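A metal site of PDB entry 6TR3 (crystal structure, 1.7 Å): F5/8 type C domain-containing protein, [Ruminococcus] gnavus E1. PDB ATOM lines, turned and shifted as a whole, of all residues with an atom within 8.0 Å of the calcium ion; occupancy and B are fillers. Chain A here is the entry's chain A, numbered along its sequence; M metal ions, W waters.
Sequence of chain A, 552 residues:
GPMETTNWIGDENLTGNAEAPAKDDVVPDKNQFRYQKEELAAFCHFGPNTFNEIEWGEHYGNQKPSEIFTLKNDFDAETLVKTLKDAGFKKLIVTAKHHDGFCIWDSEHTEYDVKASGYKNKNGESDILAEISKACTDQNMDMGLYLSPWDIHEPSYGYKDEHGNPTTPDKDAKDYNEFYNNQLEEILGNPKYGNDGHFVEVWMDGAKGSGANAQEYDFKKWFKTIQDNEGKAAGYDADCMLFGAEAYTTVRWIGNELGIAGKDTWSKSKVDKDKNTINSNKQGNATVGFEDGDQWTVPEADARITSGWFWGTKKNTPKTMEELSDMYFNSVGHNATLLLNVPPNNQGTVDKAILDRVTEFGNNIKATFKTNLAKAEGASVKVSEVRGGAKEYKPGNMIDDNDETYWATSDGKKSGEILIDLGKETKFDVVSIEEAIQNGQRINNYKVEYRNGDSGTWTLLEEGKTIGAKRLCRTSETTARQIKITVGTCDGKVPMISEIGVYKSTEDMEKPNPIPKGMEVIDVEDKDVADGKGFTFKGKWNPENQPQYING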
ATOM      1  N   GLU A 154       8.751 -12.869  22.353  1.00  0.00           N
ATOM      2  CA  GLU A 154       7.828 -13.936  21.941  1.00  0.00           C
ATOM      3  C   GLU A 154       8.544 -15.287  21.986  1.00  0.00           C
ATOM      4  O   GLU A 154       9.568 -15.465  21.327  1.00  0.00           O
ATOM      5  CB  GLU A 154       7.280 -13.644  20.533  1.00  0.00           C
ATOM      6  CG  GLU A 154       6.648 -14.809  19.812  1.00  0.00           C
ATOM      7  CD  GLU A 154       5.601 -15.547  20.636  1.00  0.00           C
ATOM      8  OE1 GLU A 154       4.888 -14.876  21.423  1.00  0.00           O
ATOM      9  OE2 GLU A 154       5.490 -16.792  20.479  1.00  0.00           O
ATOM     10  N   PRO A 155       8.065 -16.256  22.804  1.00  0.00           N
ATOM     11  CA  PRO A 155       8.767 -17.538  22.942  1.00  0.00           C
ATOM     12  C   PRO A 155       9.047 -18.301  21.662  1.00  0.00           C
ATOM     13  O   PRO A 155      10.041 -19.011  21.598  1.00  0.00           O
ATOM     14  CB  PRO A 155       7.832 -18.368  23.847  1.00  0.00           C
ATOM     15  CG  PRO A 155       6.945 -17.377  24.536  1.00  0.00           C
ATOM     16  CD  PRO A 155       6.917 -16.122  23.709  1.00  0.00           C
ATOM     17  N   SER A 156       8.186 -18.154  20.649  1.00  0.00           N
ATOM     18  CA  SER A 156       8.345 -18.861  19.403  1.00  0.00           C
ATOM     19  C   SER A 156       9.496 -18.331  18.533  1.00  0.00           C
ATOM     20  O   SER A 156       9.852 -18.969  17.560  1.00  0.00           O
ATOM     21  CB  SER A 156       7.025 -18.858  18.587  1.00  0.00           C
ATOM     22  OG  SER A 156       6.693 -17.565  18.136  1.00  0.00           O
ATOM     23  N   TYR A 157      10.049 -17.153  18.874  1.00  0.00           N
ATOM     24  CA  TYR A 157      11.176 -16.610  18.115  1.00  0.00           C
ATOM     25  C   TYR A 157      12.418 -17.484  18.305  1.00  0.00           C
ATOM     26  O   TYR A 157      12.791 -17.786  19.431  1.00  0.00           O
ATOM     27  CB  TYR A 157      11.503 -15.146  18.514  1.00  0.00           C
ATOM     28  CG  TYR A 157      12.366 -14.463  17.474  1.00  0.00           C
ATOM     29  CD1 TYR A 157      13.765 -14.525  17.524  1.00  0.00           C
ATOM     30  CD2 TYR A 157      11.783 -13.791  16.416  1.00  0.00           C
ATOM     31  CE1 TYR A 157      14.544 -13.924  16.550  1.00  0.00           C
ATOM     32  CE2 TYR A 157      12.556 -13.180  15.434  1.00  0.00           C
ATOM     33  CZ  TYR A 157      13.931 -13.249  15.497  1.00  0.00           C
ATOM     34  OH  TYR A 157      14.666 -12.625  14.513  1.00  0.00           O
ATOM     35  N   GLY A 158      13.048 -17.855  17.190  1.00  0.00           N
ATOM     36  CA  GLY A 158      14.183 -18.772  17.186  1.00  0.00           C
ATOM     37  C   GLY A 158      13.749 -20.220  17.264  1.00  0.00           C
ATOM     38  O   GLY A 158      12.555 -20.537  17.368  1.00  0.00           O
ATOM     39  N   TYR A 159      14.733 -21.119  17.226  1.00  0.00           N
ATOM     40  CA  TYR A 159      14.502 -22.551  17.169  1.00  0.00           C
ATOM     41  C   TYR A 159      14.640 -23.173  18.541  1.00  0.00           C
ATOM     42  O   TYR A 159      15.761 -23.357  19.056  1.00  0.00           O
ATOM     43  CB  TYR A 159      15.435 -23.203  16.147  1.00  0.00           C
ATOM     44  CG  TYR A 159      15.442 -22.446  14.857  1.00  0.00           C
ATOM     45  CD1 TYR A 159      14.242 -22.216  14.152  1.00  0.00           C
ATOM     46  CD2 TYR A 159      16.621 -21.929  14.336  1.00  0.00           C
ATOM     47  CE1 TYR A 159      14.246 -21.512  12.964  1.00  0.00           C
ATOM     48  CE2 TYR A 159      16.631 -21.205  13.155  1.00  0.00           C
ATOM     49  CZ  TYR A 159      15.443 -21.000  12.473  1.00  0.00           C
ATOM     50  OH  TYR A 159      15.456 -20.298  11.300  1.00  0.00           O
ATOM     51  N   LYS A 160      13.497 -23.533  19.138  1.00  0.00           N
ATOM     52  CA  LYS A 160      13.492 -24.146  20.482  1.00  0.00           C
ATOM     53  C   LYS A 160      12.549 -25.344  20.574  1.00  0.00           C
ATOM     54  O   LYS A 160      11.492 -25.373  19.941  1.00  0.00           O
ATOM     55  CB  LYS A 160      13.079 -23.120  21.534  1.00  0.00           C
ATOM     56  CG  LYS A 160      13.958 -21.891  21.636  1.00  0.00           C
ATOM     57  CD  LYS A 160      13.401 -20.923  22.672  1.00  0.00           C
ATOM     58  CE  LYS A 160      14.416 -19.844  23.016  1.00  0.00           C
ATOM     59  NZ  LYS A 160      14.811 -19.077  21.797  1.00  0.00           N
ATOM     60  N   ASP A 161      12.934 -26.306  21.418  1.00  0.00           N
ATOM     61  CA  ASP A 161      12.100 -27.453  21.737  1.00  0.00           C
ATOM     62  C   ASP A 161      10.976 -26.982  22.678  1.00  0.00           C
ATOM     63  O   ASP A 161      10.836 -25.774  22.949  1.00  0.00           O
ATOM     64  CB  ASP A 161      12.926 -28.634  22.286  1.00  0.00           C
ATOM     65  CG  ASP A 161      13.468 -28.424  23.711  1.00  0.00           C
ATOM     66  OD1 ASP A 161      13.095 -27.466  24.435  1.00  0.00           O
ATOM     67  OD2 ASP A 161      14.308 -29.239  24.086  1.00  0.00           O
ATOM     68  N   THR A 167      17.375 -25.686  19.560  1.00  0.00           N
ATOM     69  CA  THR A 167      17.401 -26.886  18.746  1.00  0.00           C
ATOM     70  C   THR A 167      17.534 -26.486  17.264  1.00  0.00           C
ATOM     71  O   THR A 167      17.762 -25.325  16.956  1.00  0.00           O
ATOM     72  CB  THR A 167      16.139 -27.739  19.009  1.00  0.00           C
ATOM     73  OG1 THR A 167      16.317 -29.042  18.441  1.00  0.00           O
ATOM     74  CG2 THR A 167      14.876 -27.063  18.442  1.00  0.00           C
ATOM     75  N   THR A 168      17.420 -27.458  16.352  1.00  0.00           N
ATOM     76  CA  THR A 168      17.496 -27.194  14.912  1.00  0.00           C
ATOM     77  C   THR A 168      16.123 -26.816  14.381  1.00  0.00           C
ATOM     78  O   THR A 168      15.111 -27.129  14.995  1.00  0.00           O
ATOM     79  CB  THR A 168      18.070 -28.384  14.153  1.00  0.00           C
ATOM     80  OG1 THR A 168      17.470 -29.593  14.621  1.00  0.00           O
ATOM     81  CG2 THR A 168      19.595 -28.477  14.395  1.00  0.00           C
ATOM     82  N   PRO A 169      16.032 -26.109  13.233  1.00  0.00           N
ATOM     83  CA  PRO A 169      14.743 -25.669  12.687  1.00  0.00           C
ATOM     84  C   PRO A 169      13.691 -26.763  12.520  1.00  0.00           C
ATOM     85  O   PRO A 169      12.509 -26.477  12.705  1.00  0.00           O
ATOM     86  CB  PRO A 169      15.129 -25.086  11.323  1.00  0.00           C
ATOM     87  CG  PRO A 169      16.531 -24.588  11.550  1.00  0.00           C
ATOM     88  CD  PRO A 169      17.170 -25.600  12.448  1.00  0.00           C
ATOM     89  N   LYS A 171      13.171 -29.280  14.409  1.00  0.00           N
ATOM     90  CA  LYS A 171      12.703 -29.735  15.719  1.00  0.00           C
ATOM     91  C   LYS A 171      12.019 -28.648  16.529  1.00  0.00           C
ATOM     92  O   LYS A 171      11.648 -28.868  17.679  1.00  0.00           O
ATOM     93  CB  LYS A 171      13.886 -30.290  16.523  1.00  0.00           C
ATOM     94  CG  LYS A 171      14.652 -31.427  15.846  1.00  0.00           C
ATOM     95  CD  LYS A 171      13.830 -32.693  15.827  1.00  0.00           C
ATOM     96  CE  LYS A 171      14.472 -33.762  14.950  1.00  0.00           C
ATOM     97  NZ  LYS A 171      15.787 -34.190  15.460  1.00  0.00           N
ATOM     98  N   ASP A 172      11.880 -27.472  15.909  1.00  0.00           N
ATOM     99  CA  ASP A 172      11.323 -26.288  16.533  1.00  0.00           C
ATOM    100  C   ASP A 172       9.834 -26.506  16.824  1.00  0.00           C
ATOM    101  O   ASP A 172       9.067 -26.823  15.923  1.00  0.00           O
ATOM    102  CB  ASP A 172      11.573 -25.108  15.587  1.00  0.00           C
ATOM    103  CG  ASP A 172      11.053 -23.792  16.119  1.00  0.00           C
ATOM    104  OD1 ASP A 172      11.151 -23.499  17.330  1.00  0.00           O
ATOM    105  OD2 ASP A 172      10.554 -23.054  15.265  1.00  0.00           O
ATOM    106  N   ALA A 173       9.446 -26.364  18.098  1.00  0.00           N
ATOM    107  CA  ALA A 173       8.119 -26.700  18.573  1.00  0.00           C
ATOM    108  C   ALA A 173       7.022 -25.664  18.230  1.00  0.00           C
ATOM    109  O   ALA A 173       5.873 -26.028  18.026  1.00  0.00           O
ATOM    110  CB  ALA A 173       8.158 -26.954  20.073  1.00  0.00           C
ATOM    111  N   LYS A 174       7.400 -24.382  18.196  1.00  0.00           N
ATOM    112  CA  LYS A 174       6.478 -23.302  17.814  1.00  0.00           C
ATOM    113  C   LYS A 174       7.126 -22.378  16.757  1.00  0.00           C
ATOM    114  O   LYS A 174       8.153 -21.762  17.025  1.00  0.00           O
ATOM    115  CB  LYS A 174       6.001 -22.507  19.028  1.00  0.00           C
ATOM    116  CG  LYS A 174       7.007 -22.412  20.173  1.00  0.00           C
ATOM    117  CD  LYS A 174       6.617 -21.435  21.286  1.00  0.00           C
ATOM    118  CE  LYS A 174       5.887 -22.111  22.430  1.00  0.00           C
ATOM    119  NZ  LYS A 174       4.534 -22.619  22.036  1.00  0.00           N
ATOM    120  N   ASP A 175       6.503 -22.302  15.587  1.00  0.00           N
ATOM    121  CA  ASP A 175       7.009 -21.538  14.443  1.00  0.00           C
ATOM    122  C   ASP A 175       6.665 -20.047  14.574  1.00  0.00           C
ATOM    123  O   ASP A 175       5.478 -19.660  14.518  1.00  0.00           O
ATOM    124  CB  ASP A 175       6.420 -22.099  13.138  1.00  0.00           C
ATOM    125  CG  ASP A 175       7.098 -21.568  11.881  1.00  0.00           C
ATOM    126  OD1 ASP A 175       7.976 -20.668  11.962  1.00  0.00           O
ATOM    127  OD2 ASP A 175       6.726 -22.070  10.794  1.00  0.00           O
ATOM    128  N   TYR A 176       7.687 -19.212  14.714  1.00  0.00           N
ATOM    129  CA  TYR A 176       7.511 -17.765  14.783  1.00  0.00           C
ATOM    130  C   TYR A 176       6.797 -17.208  13.542  1.00  0.00           C
ATOM    131  O   TYR A 176       6.039 -16.255  13.622  1.00  0.00           O
ATOM    132  CB  TYR A 176       8.855 -17.035  14.956  1.00  0.00           C
ATOM    133  CG  TYR A 176       8.721 -15.527  15.009  1.00  0.00           C
ATOM    134  CD1 TYR A 176       8.163 -14.905  16.117  1.00  0.00           C
ATOM    135  CD2 TYR A 176       9.150 -14.725  13.952  1.00  0.00           C
ATOM    136  CE1 TYR A 176       8.009 -13.526  16.163  1.00  0.00           C
ATOM    137  CE2 TYR A 176       9.008 -13.343  13.991  1.00  0.00           C
ATOM    138  CZ  TYR A 176       8.449 -12.750  15.115  1.00  0.00           C
ATOM    139  OH  TYR A 176       8.327 -11.364  15.190  1.00  0.00           O
ATOM    140  N   ASN A 177       7.069 -17.814  12.380  1.00  0.00           N
ATOM    141  CA  ASN A 177       6.386 -17.416  11.151  1.00  0.00           C
ATOM    142  C   ASN A 177       4.851 -17.487  11.253  1.00  0.00           C
ATOM    143  O   ASN A 177       4.186 -16.619  10.710  1.00  0.00           O
ATOM    144  CB  ASN A 177       6.954 -18.187   9.960  1.00  0.00           C
ATOM    145  CG  ASN A 177       8.363 -17.736   9.623  1.00  0.00           C
ATOM    146  OD1 ASN A 177       8.594 -16.550   9.391  1.00  0.00           O
ATOM    147  ND2 ASN A 177       9.316 -18.660   9.620  1.00  0.00           N
ATOM    148  N   ALA A 214      19.085 -16.922  15.535  1.00  0.00           N
ATOM    149  CA  ALA A 214      18.696 -17.077  14.141  1.00  0.00           C
ATOM    150  C   ALA A 214      17.187 -17.332  14.029  1.00  0.00           C
ATOM    151  O   ALA A 214      16.596 -17.986  14.901  1.00  0.00           O
ATOM    152  CB  ALA A 214      19.473 -18.228  13.536  1.00  0.00           C
ATOM    153  N   GLN A 215      16.582 -16.795  12.957  1.00  0.00           N
ATOM    154  CA  GLN A 215      15.178 -17.030  12.615  1.00  0.00           C
ATOM    155  C   GLN A 215      14.962 -16.664  11.150  1.00  0.00           C
ATOM    156  O   GLN A 215      15.096 -15.484  10.759  1.00  0.00           O
ATOM    157  CB  GLN A 215      14.250 -16.165  13.480  1.00  0.00           C
ATOM    158  CG  GLN A 215      12.768 -16.305  13.178  1.00  0.00           C
ATOM    159  CD  GLN A 215      12.261 -17.730  13.386  1.00  0.00           C
ATOM    160  OE1 GLN A 215      12.118 -18.190  14.517  1.00  0.00           O
ATOM    161  NE2 GLN A 215      11.957 -18.411  12.292  1.00  0.00           N
HETATM  162 CA    CA M   1      10.399 -21.107  17.018  1.00  0.00          CA
HETATM  163  O   HOH W   1      10.377 -20.208  14.853  1.00  0.00           O
HETATM  164  O   HOH W   2      10.884 -21.047  19.486  1.00  0.00           O
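Within 4 Å of the calcium ion: Ser 156, Gly 158, Asp 172 and Lys 174.
Water W1 lies within hydrogen-bond range of OE1 of Gln 215 and N of Tyr 176.
The backbone NH (N) of Gly 158 lies within hydrogen-bond range of the side-chain amide oxygen (OE1) of Gln 215, 2.8 Å away. OG of Ser 156 lies within hydrogen-bond range of OE2 of Glu 154, 2.7 Å away. N of Lys 160 lies close to OD1 of Asp 172, 3.0 Å away.
The calcium ion is bound by O of Gly 158 (2.3 Å), O of Ser 156 (2.3 Å), O of Lys 174 (2.3 Å), water W1 (2.3 Å), water W2 (2.5 Å), OD1 of Asp 172 (2.5 Å) and OD2 of Asp 172 (2.6 Å). The calcium ion has seven donor atoms within binding distance.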
